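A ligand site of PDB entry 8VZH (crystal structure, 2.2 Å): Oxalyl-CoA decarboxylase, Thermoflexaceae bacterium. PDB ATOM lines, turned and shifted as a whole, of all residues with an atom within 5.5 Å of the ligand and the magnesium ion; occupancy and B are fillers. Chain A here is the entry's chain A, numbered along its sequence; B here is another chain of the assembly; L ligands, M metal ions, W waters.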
ATOM      1  N   TYR A 367       9.396 -25.399 -29.851  1.00  0.00           N
ATOM      2  CA  TYR A 367       9.015 -26.671 -29.231  1.00  0.00           C
ATOM      3  C   TYR A 367       8.729 -27.735 -30.289  1.00  0.00           C
ATOM      4  O   TYR A 367       9.218 -28.876 -30.187  1.00  0.00           O
ATOM      5  CB  TYR A 367       7.787 -26.473 -28.348  1.00  0.00           C
ATOM      6  CG  TYR A 367       8.042 -25.755 -27.034  1.00  0.00           C
ATOM      7  CD1 TYR A 367       8.496 -26.453 -25.920  1.00  0.00           C
ATOM      8  CD2 TYR A 367       7.798 -24.395 -26.905  1.00  0.00           C
ATOM      9  CE1 TYR A 367       8.706 -25.804 -24.712  1.00  0.00           C
ATOM     10  CE2 TYR A 367       8.000 -23.741 -25.708  1.00  0.00           C
ATOM     11  CZ  TYR A 367       8.459 -24.448 -24.621  1.00  0.00           C
ATOM     12  OH  TYR A 367       8.671 -23.803 -23.426  1.00  0.00           O
ATOM     13  N   GLU A 387       7.483 -33.309 -18.112  1.00  0.00           N
ATOM     14  CA  GLU A 387       7.243 -32.431 -16.976  1.00  0.00           C
ATOM     15  C   GLU A 387       7.622 -31.002 -17.307  1.00  0.00           C
ATOM     16  O   GLU A 387       8.650 -30.751 -17.941  1.00  0.00           O
ATOM     17  CB  GLU A 387       8.038 -32.897 -15.740  1.00  0.00           C
ATOM     18  CG  GLU A 387       7.747 -32.104 -14.480  1.00  0.00           C
ATOM     19  CD  GLU A 387       8.741 -32.377 -13.361  1.00  0.00           C
ATOM     20  OE1 GLU A 387       9.915 -32.724 -13.663  1.00  0.00           O
ATOM     21  OE2 GLU A 387       8.368 -32.244 -12.175  1.00  0.00           O
ATOM     22  N   GLY A 388       6.814 -30.059 -16.845  1.00  0.00           N
ATOM     23  CA  GLY A 388       7.073 -28.662 -17.136  1.00  0.00           C
ATOM     24  C   GLY A 388       5.774 -27.935 -17.423  1.00  0.00           C
ATOM     25  O   GLY A 388       4.718 -28.363 -16.964  1.00  0.00           O
ATOM     26  N   ALA A 389       5.843 -26.836 -18.165  1.00  0.00           N
ATOM     27  CA  ALA A 389       4.623 -26.132 -18.529  1.00  0.00           C
ATOM     28  C   ALA A 389       4.412 -26.350 -20.012  1.00  0.00           C
ATOM     29  O   ALA A 389       3.763 -27.346 -20.403  1.00  0.00           O
ATOM     30  CB  ALA A 389       4.686 -24.650 -18.113  1.00  0.00           C
ATOM     31  N   SER A 390       4.949 -25.496 -20.891  1.00  0.00           N
ATOM     32  CA  SER A 390       4.805 -25.739 -22.331  1.00  0.00           C
ATOM     33  C   SER A 390       5.513 -27.022 -22.747  1.00  0.00           C
ATOM     34  O   SER A 390       5.018 -27.756 -23.610  1.00  0.00           O
ATOM     35  CB  SER A 390       5.327 -24.555 -23.124  1.00  0.00           C
ATOM     36  OG  SER A 390       4.531 -23.403 -22.900  1.00  0.00           O
ATOM     37  N   THR A 391       6.676 -27.310 -22.158  1.00  0.00           N
ATOM     38  CA  THR A 391       7.364 -28.563 -22.452  1.00  0.00           C
ATOM     39  C   THR A 391       6.442 -29.771 -22.252  1.00  0.00           C
ATOM     40  O   THR A 391       6.451 -30.716 -23.053  1.00  0.00           O
ATOM     41  CB  THR A 391       8.616 -28.702 -21.585  1.00  0.00           C
ATOM     42  OG1 THR A 391       9.564 -27.685 -21.938  1.00  0.00           O
ATOM     43  CG2 THR A 391       9.262 -30.067 -21.775  1.00  0.00           C
ATOM     44  N   PHE A 413      -2.210 -32.770  -9.573  1.00  0.00           N
ATOM     45  CA  PHE A 413      -1.689 -31.724  -8.700  1.00  0.00           C
ATOM     46  C   PHE A 413      -0.807 -30.720  -9.445  1.00  0.00           C
ATOM     47  O   PHE A 413      -0.381 -29.743  -8.831  1.00  0.00           O
ATOM     48  CB  PHE A 413      -0.883 -32.350  -7.554  1.00  0.00           C
ATOM     49  CG  PHE A 413      -1.155 -31.736  -6.202  1.00  0.00           C
ATOM     50  CD1 PHE A 413      -2.309 -31.012  -5.973  1.00  0.00           C
ATOM     51  CD2 PHE A 413      -0.238 -31.892  -5.165  1.00  0.00           C
ATOM     52  CE1 PHE A 413      -2.556 -30.455  -4.735  1.00  0.00           C
ATOM     53  CE2 PHE A 413      -0.483 -31.345  -3.923  1.00  0.00           C
ATOM     54  CZ  PHE A 413      -1.645 -30.615  -3.705  1.00  0.00           C
ATOM     55  N   GLY A 414      -0.521 -30.938 -10.725  1.00  0.00           N
ATOM     56  CA  GLY A 414       0.360 -30.033 -11.445  1.00  0.00           C
ATOM     57  C   GLY A 414       1.711 -29.851 -10.793  1.00  0.00           C
ATOM     58  O   GLY A 414       2.246 -28.738 -10.768  1.00  0.00           O
ATOM     59  N   THR A 415       2.280 -30.931 -10.267  1.00  0.00           N
ATOM     60  CA  THR A 415       3.468 -30.847  -9.438  1.00  0.00           C
ATOM     61  C   THR A 415       4.732 -30.749 -10.297  1.00  0.00           C
ATOM     62  O   THR A 415       4.973 -31.600 -11.148  1.00  0.00           O
ATOM     63  CB  THR A 415       3.554 -32.078  -8.544  1.00  0.00           C
ATOM     64  OG1 THR A 415       2.291 -32.273  -7.895  1.00  0.00           O
ATOM     65  CG2 THR A 415       4.650 -31.917  -7.509  1.00  0.00           C
ATOM     66  N   MET A 416       5.540 -29.716 -10.047  1.00  0.00           N
ATOM     67  CA  MET A 416       6.922 -29.713 -10.485  1.00  0.00           C
ATOM     68  C   MET A 416       7.770 -30.416  -9.427  1.00  0.00           C
ATOM     69  O   MET A 416       7.559 -30.234  -8.227  1.00  0.00           O
ATOM     70  CB  MET A 416       7.445 -28.291 -10.705  1.00  0.00           C
ATOM     71  CG  MET A 416       6.802 -27.548 -11.860  1.00  0.00           C
ATOM     72  SD  MET A 416       6.981 -28.412 -13.434  1.00  0.00           S
ATOM     73  CE  MET A 416       5.341 -29.132 -13.641  1.00  0.00           C
ATOM     74  N   GLN A 439      11.937 -32.747 -19.811  1.00  0.00           N
ATOM     75  CA  GLN A 439      11.576 -31.704 -18.870  1.00  0.00           C
ATOM     76  C   GLN A 439      11.932 -30.334 -19.413  1.00  0.00           C
ATOM     77  O   GLN A 439      12.894 -30.176 -20.180  1.00  0.00           O
ATOM     78  CB  GLN A 439      12.290 -31.879 -17.532  1.00  0.00           C
ATOM     79  CG  GLN A 439      12.047 -33.200 -16.856  1.00  0.00           C
ATOM     80  CD  GLN A 439      12.982 -33.393 -15.690  1.00  0.00           C
ATOM     81  OE1 GLN A 439      12.597 -33.230 -14.538  1.00  0.00           O
ATOM     82  NE2 GLN A 439      14.232 -33.724 -15.991  1.00  0.00           N
ATOM     83  N   GLY A 440      11.160 -29.334 -18.993  1.00  0.00           N
ATOM     84  CA  GLY A 440      11.605 -27.962 -19.129  1.00  0.00           C
ATOM     85  C   GLY A 440      12.749 -27.659 -18.176  1.00  0.00           C
ATOM     86  O   GLY A 440      12.980 -28.374 -17.195  1.00  0.00           O
ATOM     87  N   ASP A 441      13.489 -26.590 -18.477  1.00  0.00           N
ATOM     88  CA  ASP A 441      14.683 -26.308 -17.674  1.00  0.00           C
ATOM     89  C   ASP A 441      14.326 -26.091 -16.203  1.00  0.00           C
ATOM     90  O   ASP A 441      15.009 -26.608 -15.317  1.00  0.00           O
ATOM     91  CB  ASP A 441      15.447 -25.103 -18.241  1.00  0.00           C
ATOM     92  CG  ASP A 441      14.583 -23.860 -18.420  1.00  0.00           C
ATOM     93  OD1 ASP A 441      13.538 -23.929 -19.107  1.00  0.00           O
ATOM     94  OD2 ASP A 441      14.977 -22.801 -17.891  1.00  0.00           O
ATOM     95  N   SER A 442      13.235 -25.373 -15.937  1.00  0.00           N
ATOM     96  CA  SER A 442      12.817 -25.175 -14.546  1.00  0.00           C
ATOM     97  C   SER A 442      12.467 -26.500 -13.881  1.00  0.00           C
ATOM     98  O   SER A 442      12.884 -26.778 -12.751  1.00  0.00           O
ATOM     99  CB  SER A 442      11.636 -24.209 -14.475  1.00  0.00           C
ATOM    100  OG  SER A 442      11.255 -23.990 -13.137  1.00  0.00           O
ATOM    101  N   ALA A 443      11.668 -27.321 -14.575  1.00  0.00           N
ATOM    102  CA  ALA A 443      11.295 -28.627 -14.025  1.00  0.00           C
ATOM    103  C   ALA A 443      12.534 -29.431 -13.678  1.00  0.00           C
ATOM    104  O   ALA A 443      12.591 -30.066 -12.619  1.00  0.00           O
ATOM    105  CB  ALA A 443      10.420 -29.392 -15.030  1.00  0.00           C
ATOM    106  N   PHE A 444      13.547 -29.409 -14.550  1.00  0.00           N
ATOM    107  CA  PHE A 444      14.733 -30.201 -14.292  1.00  0.00           C
ATOM    108  C   PHE A 444      15.416 -29.802 -12.993  1.00  0.00           C
ATOM    109  O   PHE A 444      16.010 -30.651 -12.318  1.00  0.00           O
ATOM    110  CB  PHE A 444      15.720 -30.095 -15.460  1.00  0.00           C
ATOM    111  CG  PHE A 444      17.019 -30.780 -15.208  1.00  0.00           C
ATOM    112  CD1 PHE A 444      17.127 -32.160 -15.317  1.00  0.00           C
ATOM    113  CD2 PHE A 444      18.144 -30.058 -14.823  1.00  0.00           C
ATOM    114  CE1 PHE A 444      18.325 -32.814 -15.071  1.00  0.00           C
ATOM    115  CE2 PHE A 444      19.351 -30.694 -14.566  1.00  0.00           C
ATOM    116  CZ  PHE A 444      19.438 -32.072 -14.687  1.00  0.00           C
ATOM    117  N   PHE A 446      14.186 -28.911 -10.148  1.00  0.00           N
ATOM    118  CA  PHE A 446      13.524 -29.312  -8.902  1.00  0.00           C
ATOM    119  C   PHE A 446      14.143 -30.564  -8.311  1.00  0.00           C
ATOM    120  O   PHE A 446      14.130 -30.732  -7.084  1.00  0.00           O
ATOM    121  CB  PHE A 446      12.037 -29.532  -9.130  1.00  0.00           C
ATOM    122  CG  PHE A 446      11.224 -28.270  -9.072  1.00  0.00           C
ATOM    123  CD1 PHE A 446      11.203 -27.408 -10.153  1.00  0.00           C
ATOM    124  CD2 PHE A 446      10.491 -27.956  -7.934  1.00  0.00           C
ATOM    125  CE1 PHE A 446      10.452 -26.245 -10.106  1.00  0.00           C
ATOM    126  CE2 PHE A 446       9.740 -26.793  -7.887  1.00  0.00           C
ATOM    127  CZ  PHE A 446       9.714 -25.944  -8.971  1.00  0.00           C
ATOM    128  N   ILE A 466      14.520 -29.179 -22.175  1.00  0.00           N
ATOM    129  CA  ILE A 466      14.105 -28.204 -23.175  1.00  0.00           C
ATOM    130  C   ILE A 466      14.186 -26.845 -22.505  1.00  0.00           C
ATOM    131  O   ILE A 466      13.395 -26.528 -21.597  1.00  0.00           O
ATOM    132  CB  ILE A 466      12.711 -28.522 -23.724  1.00  0.00           C
ATOM    133  CG1 ILE A 466      12.783 -29.803 -24.564  1.00  0.00           C
ATOM    134  CG2 ILE A 466      12.175 -27.346 -24.516  1.00  0.00           C
ATOM    135  CD1 ILE A 466      11.479 -30.225 -25.184  1.00  0.00           C
ATOM    136  N   ASN A 467      15.149 -26.020 -22.921  1.00  0.00           N
ATOM    137  CA  ASN A 467      15.684 -24.947 -22.100  1.00  0.00           C
ATOM    138  C   ASN A 467      15.441 -23.607 -22.780  1.00  0.00           C
ATOM    139  O   ASN A 467      16.119 -23.270 -23.761  1.00  0.00           O
ATOM    140  CB  ASN A 467      17.172 -25.194 -21.850  1.00  0.00           C
ATOM    141  CG  ASN A 467      17.778 -24.218 -20.857  1.00  0.00           C
ATOM    142  OD1 ASN A 467      17.164 -23.221 -20.475  1.00  0.00           O
ATOM    143  ND2 ASN A 467      19.021 -24.489 -20.447  1.00  0.00           N
ATOM    144  N   ASN A 468      14.485 -22.832 -22.252  1.00  0.00           N
ATOM    145  CA  ASN A 468      14.234 -21.467 -22.707  1.00  0.00           C
ATOM    146  C   ASN A 468      14.690 -20.425 -21.687  1.00  0.00           C
ATOM    147  O   ASN A 468      14.242 -19.267 -21.733  1.00  0.00           O
ATOM    148  CB  ASN A 468      12.759 -21.263 -23.054  1.00  0.00           C
ATOM    149  CG  ASN A 468      11.826 -21.690 -21.939  1.00  0.00           C
ATOM    150  OD1 ASN A 468      12.249 -21.933 -20.805  1.00  0.00           O
ATOM    151  ND2 ASN A 468      10.535 -21.781 -22.248  1.00  0.00           N
ATOM    152  N   ASN A 469      15.557 -20.821 -20.747  1.00  0.00           N
ATOM    153  CA  ASN A 469      16.181 -19.949 -19.754  1.00  0.00           C
ATOM    154  C   ASN A 469      15.250 -19.537 -18.623  1.00  0.00           C
ATOM    155  O   ASN A 469      15.487 -18.513 -17.983  1.00  0.00           O
ATOM    156  CB  ASN A 469      16.772 -18.668 -20.377  1.00  0.00           C
ATOM    157  CG  ASN A 469      17.982 -18.951 -21.243  1.00  0.00           C
ATOM    158  OD1 ASN A 469      18.653 -19.961 -21.091  1.00  0.00           O
ATOM    159  ND2 ASN A 469      18.267 -18.034 -22.166  1.00  0.00           N
ATOM    160  N   GLY A 470      14.188 -20.290 -18.345  1.00  0.00           N
ATOM    161  CA  GLY A 470      13.409 -19.983 -17.168  1.00  0.00           C
ATOM    162  C   GLY A 470      12.021 -20.618 -17.191  1.00  0.00           C
ATOM    163  O   GLY A 470      11.753 -21.545 -17.966  1.00  0.00           O
ATOM    164  N   ILE A 471      11.178 -20.102 -16.304  1.00  0.00           N
ATOM    165  CA  ILE A 471       9.799 -20.556 -16.127  1.00  0.00           C
ATOM    166  C   ILE A 471       8.969 -19.858 -17.211  1.00  0.00           C
ATOM    167  O   ILE A 471       8.638 -18.680 -17.085  1.00  0.00           O
ATOM    168  CB  ILE A 471       9.273 -20.246 -14.724  1.00  0.00           C
ATOM    169  CG1 ILE A 471      10.127 -20.972 -13.673  1.00  0.00           C
ATOM    170  CG2 ILE A 471       7.819 -20.642 -14.588  1.00  0.00           C
ATOM    171  CD1 ILE A 471       9.824 -20.564 -12.246  1.00  0.00           C
ATOM    172  N   GLY A 472       8.640 -20.587 -18.272  1.00  0.00           N
ATOM    173  CA  GLY A 472       8.034 -19.942 -19.418  1.00  0.00           C
ATOM    174  C   GLY A 472       8.979 -19.068 -20.200  1.00  0.00           C
ATOM    175  O   GLY A 472       8.529 -18.311 -21.060  1.00  0.00           O
ATOM    176  N   GLY A 473      10.254 -19.141 -19.916  1.00  0.00           N
ATOM    177  CA  GLY A 473      11.233 -18.410 -20.691  1.00  0.00           C
ATOM    178  C   GLY A 473      11.959 -17.366 -19.879  1.00  0.00           C
ATOM    179  O   GLY A 473      11.406 -16.774 -18.941  1.00  0.00           O
ATOM    180  N   ILE A 534      15.923 -23.577 -26.735  1.00  0.00           N
ATOM    181  CA  ILE A 534      14.811 -23.150 -27.571  1.00  0.00           C
ATOM    182  C   ILE A 534      14.569 -21.664 -27.332  1.00  0.00           C
ATOM    183  O   ILE A 534      15.073 -21.068 -26.378  1.00  0.00           O
ATOM    184  CB  ILE A 534      13.527 -23.969 -27.320  1.00  0.00           C
ATOM    185  CG1 ILE A 534      13.167 -23.931 -25.837  1.00  0.00           C
ATOM    186  CG2 ILE A 534      13.686 -25.399 -27.810  1.00  0.00           C
ATOM    187  CD1 ILE A 534      11.685 -23.898 -25.572  1.00  0.00           C
ATOM    188  N   ILE B  25       9.398 -19.665  -5.610  1.00  0.00           N
ATOM    189  CA  ILE B  25       9.310 -20.003  -7.017  1.00  0.00           C
ATOM    190  C   ILE B  25       7.960 -19.517  -7.522  1.00  0.00           C
ATOM    191  O   ILE B  25       6.925 -19.842  -6.941  1.00  0.00           O
ATOM    192  CB  ILE B  25       9.477 -21.514  -7.253  1.00  0.00           C
ATOM    193  CG1 ILE B  25      10.828 -21.988  -6.713  1.00  0.00           C
ATOM    194  CG2 ILE B  25       9.323 -21.850  -8.733  1.00  0.00           C
ATOM    195  CD1 ILE B  25      11.106 -23.456  -6.921  1.00  0.00           C
ATOM    196  N   VAL B  26       7.979 -18.735  -8.608  1.00  0.00           N
ATOM    197  CA  VAL B  26       6.757 -18.099  -9.071  1.00  0.00           C
ATOM    198  C   VAL B  26       5.913 -19.079  -9.880  1.00  0.00           C
ATOM    199  O   VAL B  26       6.386 -20.110 -10.367  1.00  0.00           O
ATOM    200  CB  VAL B  26       7.058 -16.832  -9.900  1.00  0.00           C
ATOM    201  CG1 VAL B  26       7.666 -15.754  -9.014  1.00  0.00           C
ATOM    202  CG2 VAL B  26       7.964 -17.178 -11.072  1.00  0.00           C
ATOM    203  N   GLY B  27       4.661 -18.715 -10.057  1.00  0.00           N
ATOM    204  CA  GLY B  27       3.668 -19.544 -10.693  1.00  0.00           C
ATOM    205  C   GLY B  27       2.297 -19.114 -10.227  1.00  0.00           C
ATOM    206  O   GLY B  27       2.155 -18.355  -9.269  1.00  0.00           O
ATOM    207  N   ILE B  28       1.286 -19.589 -10.950  1.00  0.00           N
ATOM    208  CA  ILE B  28      -0.100 -19.302 -10.577  1.00  0.00           C
ATOM    209  C   ILE B  28      -0.306 -19.708  -9.119  1.00  0.00           C
ATOM    210  O   ILE B  28       0.027 -20.835  -8.741  1.00  0.00           O
ATOM    211  CB  ILE B  28      -1.081 -20.056 -11.491  1.00  0.00           C
ATOM    212  CG1 ILE B  28      -0.764 -19.772 -12.957  1.00  0.00           C
ATOM    213  CG2 ILE B  28      -2.515 -19.675 -11.156  1.00  0.00           C
ATOM    214  CD1 ILE B  28      -1.617 -20.553 -13.930  1.00  0.00           C
ATOM    215  N   GLU B  50      11.112 -25.110  -3.636  1.00  0.00           N
ATOM    216  CA  GLU B  50      10.593 -24.352  -2.497  1.00  0.00           C
ATOM    217  C   GLU B  50      11.115 -24.874  -1.171  1.00  0.00           C
ATOM    218  O   GLU B  50      11.111 -24.128  -0.176  1.00  0.00           O
ATOM    219  CB  GLU B  50       9.067 -24.375  -2.455  1.00  0.00           C
ATOM    220  CG  GLU B  50       8.403 -23.720  -3.631  1.00  0.00           C
ATOM    221  CD  GLU B  50       8.230 -24.661  -4.798  1.00  0.00           C
ATOM    222  OE1 GLU B  50       8.700 -25.808  -4.706  1.00  0.00           O
ATOM    223  OE2 GLU B  50       7.620 -24.245  -5.796  1.00  0.00           O
ATOM    224  N   VAL B  73       3.573 -21.406  -4.675  1.00  0.00           N
ATOM    225  CA  VAL B  73       2.321 -21.568  -5.414  1.00  0.00           C
ATOM    226  C   VAL B  73       1.375 -22.446  -4.616  1.00  0.00           C
ATOM    227  O   VAL B  73       1.735 -23.022  -3.589  1.00  0.00           O
ATOM    228  CB  VAL B  73       2.559 -22.173  -6.812  1.00  0.00           C
ATOM    229  CG1 VAL B  73       3.550 -21.334  -7.597  1.00  0.00           C
ATOM    230  CG2 VAL B  73       3.027 -23.626  -6.697  1.00  0.00           C
ATOM    231  N   PRO B  76       1.120 -28.215  -4.273  1.00  0.00           N
ATOM    232  CA  PRO B  76       2.448 -28.799  -4.026  1.00  0.00           C
ATOM    233  C   PRO B  76       3.521 -27.773  -3.703  1.00  0.00           C
ATOM    234  O   PRO B  76       4.495 -28.102  -3.029  1.00  0.00           O
ATOM    235  CB  PRO B  76       2.748 -29.551  -5.328  1.00  0.00           C
ATOM    236  CG  PRO B  76       1.940 -28.843  -6.365  1.00  0.00           C
ATOM    237  CD  PRO B  76       0.681 -28.403  -5.664  1.00  0.00           C
ATOM    238  N   GLY B  77       3.373 -26.524  -4.178  1.00  0.00           N
ATOM    239  CA  GLY B  77       4.361 -25.514  -3.850  1.00  0.00           C
ATOM    240  C   GLY B  77       4.355 -25.179  -2.369  1.00  0.00           C
ATOM    241  O   GLY B  77       5.411 -25.137  -1.732  1.00  0.00           O
ATOM    242  N   HIS B  80       5.792 -28.303  -0.341  1.00  0.00           N
ATOM    243  CA  HIS B  80       7.252 -28.232  -0.274  1.00  0.00           C
ATOM    244  C   HIS B  80       7.720 -27.228   0.784  1.00  0.00           C
ATOM    245  O   HIS B  80       8.749 -27.444   1.439  1.00  0.00           O
ATOM    246  CB  HIS B  80       7.824 -27.838  -1.639  1.00  0.00           C
ATOM    247  CG  HIS B  80       7.619 -28.869  -2.708  1.00  0.00           C
ATOM    248  ND1 HIS B  80       8.060 -28.691  -3.998  1.00  0.00           N
ATOM    249  CD2 HIS B  80       7.022 -30.081  -2.674  1.00  0.00           C
ATOM    250  CE1 HIS B  80       7.748 -29.759  -4.720  1.00  0.00           C
ATOM    251  NE2 HIS B  80       7.112 -30.614  -3.941  1.00  0.00           N
ATOM    252  N   PHE B 112      -7.609 -26.372  -9.706  1.00  0.00           N
ATOM    253  CA  PHE B 112      -6.191 -26.590  -9.908  1.00  0.00           C
ATOM    254  C   PHE B 112      -5.435 -26.377  -8.596  1.00  0.00           C
ATOM    255  O   PHE B 112      -5.478 -25.297  -8.002  1.00  0.00           O
ATOM    256  CB  PHE B 112      -5.676 -25.652 -10.992  1.00  0.00           C
ATOM    257  CG  PHE B 112      -4.216 -25.821 -11.292  1.00  0.00           C
ATOM    258  CD1 PHE B 112      -3.751 -27.012 -11.827  1.00  0.00           C
ATOM    259  CD2 PHE B 112      -3.317 -24.802 -11.036  1.00  0.00           C
ATOM    260  CE1 PHE B 112      -2.411 -27.176 -12.105  1.00  0.00           C
ATOM    261  CE2 PHE B 112      -1.979 -24.956 -11.318  1.00  0.00           C
ATOM    262  CZ  PHE B 112      -1.523 -26.146 -11.847  1.00  0.00           C
ATOM    263  N   GLN B 113      -4.775 -27.441  -8.134  1.00  0.00           N
ATOM    264  CA  GLN B 113      -3.961 -27.401  -6.915  1.00  0.00           C
ATOM    265  C   GLN B 113      -4.780 -27.047  -5.677  1.00  0.00           C
ATOM    266  O   GLN B 113      -4.264 -26.438  -4.724  1.00  0.00           O
ATOM    267  CB  GLN B 113      -2.761 -26.469  -7.104  1.00  0.00           C
ATOM    268  CG  GLN B 113      -1.799 -27.017  -8.149  1.00  0.00           C
ATOM    269  CD  GLN B 113      -0.611 -26.131  -8.400  1.00  0.00           C
ATOM    270  OE1 GLN B 113      -0.650 -24.933  -8.115  1.00  0.00           O
ATOM    271  NE2 GLN B 113       0.453 -26.712  -8.933  1.00  0.00           N
HETATM  272  N1  LIG L   1       6.234 -25.372  -7.734  1.00  0.00           N
HETATM  273  C1  LIG L   1       5.568 -26.539  -7.779  1.00  0.00           C
HETATM  274  C2  LIG L   1       5.852 -27.540  -6.720  1.00  0.00           C
HETATM  275  N2  LIG L   1       4.671 -26.873  -8.716  1.00  0.00           N
HETATM  276  C3  LIG L   1       4.396 -25.979  -9.686  1.00  0.00           C
HETATM  277  N3  LIG L   1       3.502 -26.336 -10.600  1.00  0.00           N
HETATM  278  C4  LIG L   1       5.060 -24.710  -9.719  1.00  0.00           C
HETATM  279  C5  LIG L   1       5.963 -24.496  -8.698  1.00  0.00           C
HETATM  280  C6  LIG L   1       4.806 -23.680 -10.775  1.00  0.00           C
HETATM  281  N4  LIG L   1       5.225 -24.113 -12.128  1.00  0.00           N
HETATM  282  C7  LIG L   1       4.401 -24.585 -13.037  1.00  0.00           C
HETATM  283  S1  LIG L   1       5.181 -25.001 -14.458  1.00  0.00           S
HETATM  284  C8  LIG L   1       6.700 -24.514 -13.806  1.00  0.00           C
HETATM  285  C9  LIG L   1       6.556 -24.066 -12.536  1.00  0.00           C
HETATM  286  C10 LIG L   1       7.627 -23.557 -11.632  1.00  0.00           C
HETATM  287  C11 LIG L   1       7.953 -24.631 -14.627  1.00  0.00           C
HETATM  288  C12 LIG L   1       7.785 -24.087 -16.031  1.00  0.00           C
HETATM  289  O1  LIG L   1       9.097 -23.964 -16.641  1.00  0.00           O
HETATM  290  P1  LIG L   1       9.808 -25.123 -17.436  1.00  0.00           P
HETATM  291  O2  LIG L   1       9.845 -26.381 -16.654  1.00  0.00           O
HETATM  292  O3  LIG L   1      11.169 -24.632 -17.891  1.00  0.00           O
HETATM  293  O4  LIG L   1       8.893 -25.179 -18.706  1.00  0.00           O
HETATM  294  P2  LIG L   1       8.588 -24.322 -20.002  1.00  0.00           P
HETATM  295  O5  LIG L   1       8.858 -25.101 -21.240  1.00  0.00           O
HETATM  296  O6  LIG L   1       7.151 -23.859 -19.830  1.00  0.00           O
HETATM  297  O7  LIG L   1       9.503 -23.085 -19.844  1.00  0.00           O
HETATM  298 MG    MG M   1      11.520 -23.205 -19.358  1.00  0.00          MG
HETATM  299  O   HOH W   1      11.604 -24.719 -20.973  1.00  0.00           O
HETATM  300  O   HOH W   2       1.337 -24.213 -12.112  1.00  0.00           O
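An oxygen (O6) of the ligand lies within hydrogen-bond range of the backbone NH (N) of Ser 390, at 2.9 Å. N of Gly 472 sits close to O7 of the ligand (3.1 Å). A nitrogen (N3) of the ligand lies within hydrogen-bond range of the backbone carbonyl oxygen of Gly 414. The backbone NH of Met 416 is in hydrogen-bond range of a nitrogen (N2) of the ligand (3.3 Å). OG1 of Thr 391 sits at hydrogen-bond distance from O5 of the ligand (2.8 Å). A nitrogen (N3) of the ligand lies close to the side-chain amide nitrogen of Gln 113 of chain B (3.5 Å). N of Ala 443 sits at hydrogen-bond distance from O2 of the ligand, 2.9 Å away. O5 of the ligand sits at hydrogen-bond distance from N of Thr 391 (3.2 Å). O3 of the ligand lies close to N of Ser 442 (2.9 Å). A nitrogen (N1) of the ligand sits at hydrogen-bond distance from the side-chain carboxylate (OE2) of Glu 50 of chain B, at 2.6 Å. O3 of the ligand sits close to N of Asp 441, 3.1 Å away. An oxygen (O5) of the ligand lies within hydrogen-bond range of the side-chain hydroxyl (OH) of Tyr 367 (2.5 Å).
The backbone NH of Gly 440 sits at hydrogen-bond distance from the backbone carbonyl oxygen of Glu 387, at 3.1 Å. The side-chain amide nitrogen of Asn 468 sits at hydrogen-bond distance from the side-chain hydroxyl of Tyr 367 (3.0 Å). N of Asp 441 is in hydrogen-bond range of O of Ile 466 (3.1 Å). The side-chain sulfur (SD) of Met 416 sits close to the backbone NH (N) of Gly 388 (3.8 Å). O of Gly 414 lies within hydrogen-bond range of NE2 of Gln 113 of chain B (3.3 Å). The side-chain amide nitrogen (NE2) of Gln 113 of chain B sits at hydrogen-bond distance from the backbone carbonyl oxygen (O) of Phe 413 (3.1 Å). The side-chain carboxylate (OD2) of Asp 441 sits close to the side-chain amide oxygen (OD1) of Asn 467, at 3.4 Å. The side-chain carboxylate (OE1) of Glu 50 of chain B is in hydrogen-bond range of a ring nitrogen (ND1) of His 80 of chain B, 3.0 Å away.
Gly 388 touches the ligand (CA to O2, 3.6 Å). Ala 389 touches the ligand. Gly 440 touches the ligand. CZ of Phe 446 touches N1 of the ligand, at 3.7 Å. Ile 471 touches the ligand. CG2 of Ile 25 of chain B touches C10 of the ligand (3.8 Å). Val 26 of chain B touches the ligand (O to C10, 3.9 Å). Val 73 of chain B touches the ligand (CG2 to C5, 3.7 Å). Pro 76 of chain B touches the ligand (C to C2, 3.8 Å). Gly 77 of chain B touches the ligand. His 80 of chain B touches the ligand. Hydrophobic or aromatic side chains that line the ligand: Tyr 367, Ala 389, Met 416, Ala 443, Phe 446, Ile 471, Ile 25 of chain B, Val 73 of chain B, Pro 76 of chain B and His 80 of chain B. Of the 37 residues printed, 24 come within 4 Å of the ligand. The nearest printed residue that does not touch the ligand is Gly 473 (4.02 Å).
The magnesium ion is bound by OD1 of Asn 468 (2.1 Å), O3 of the ligand (2.1 Å), O7 of the ligand (2.1 Å), OD1 of Asp 441 (2.2 Å), O of Gly 470 (2.2 Å) and water W1 (2.2 Å).
Water W1 lies within hydrogen-bond range of O of Ile 466 (2.6 Å), O5 of the ligand (2.8 Å) and ND2 of Asn 468 (3.4 Å).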
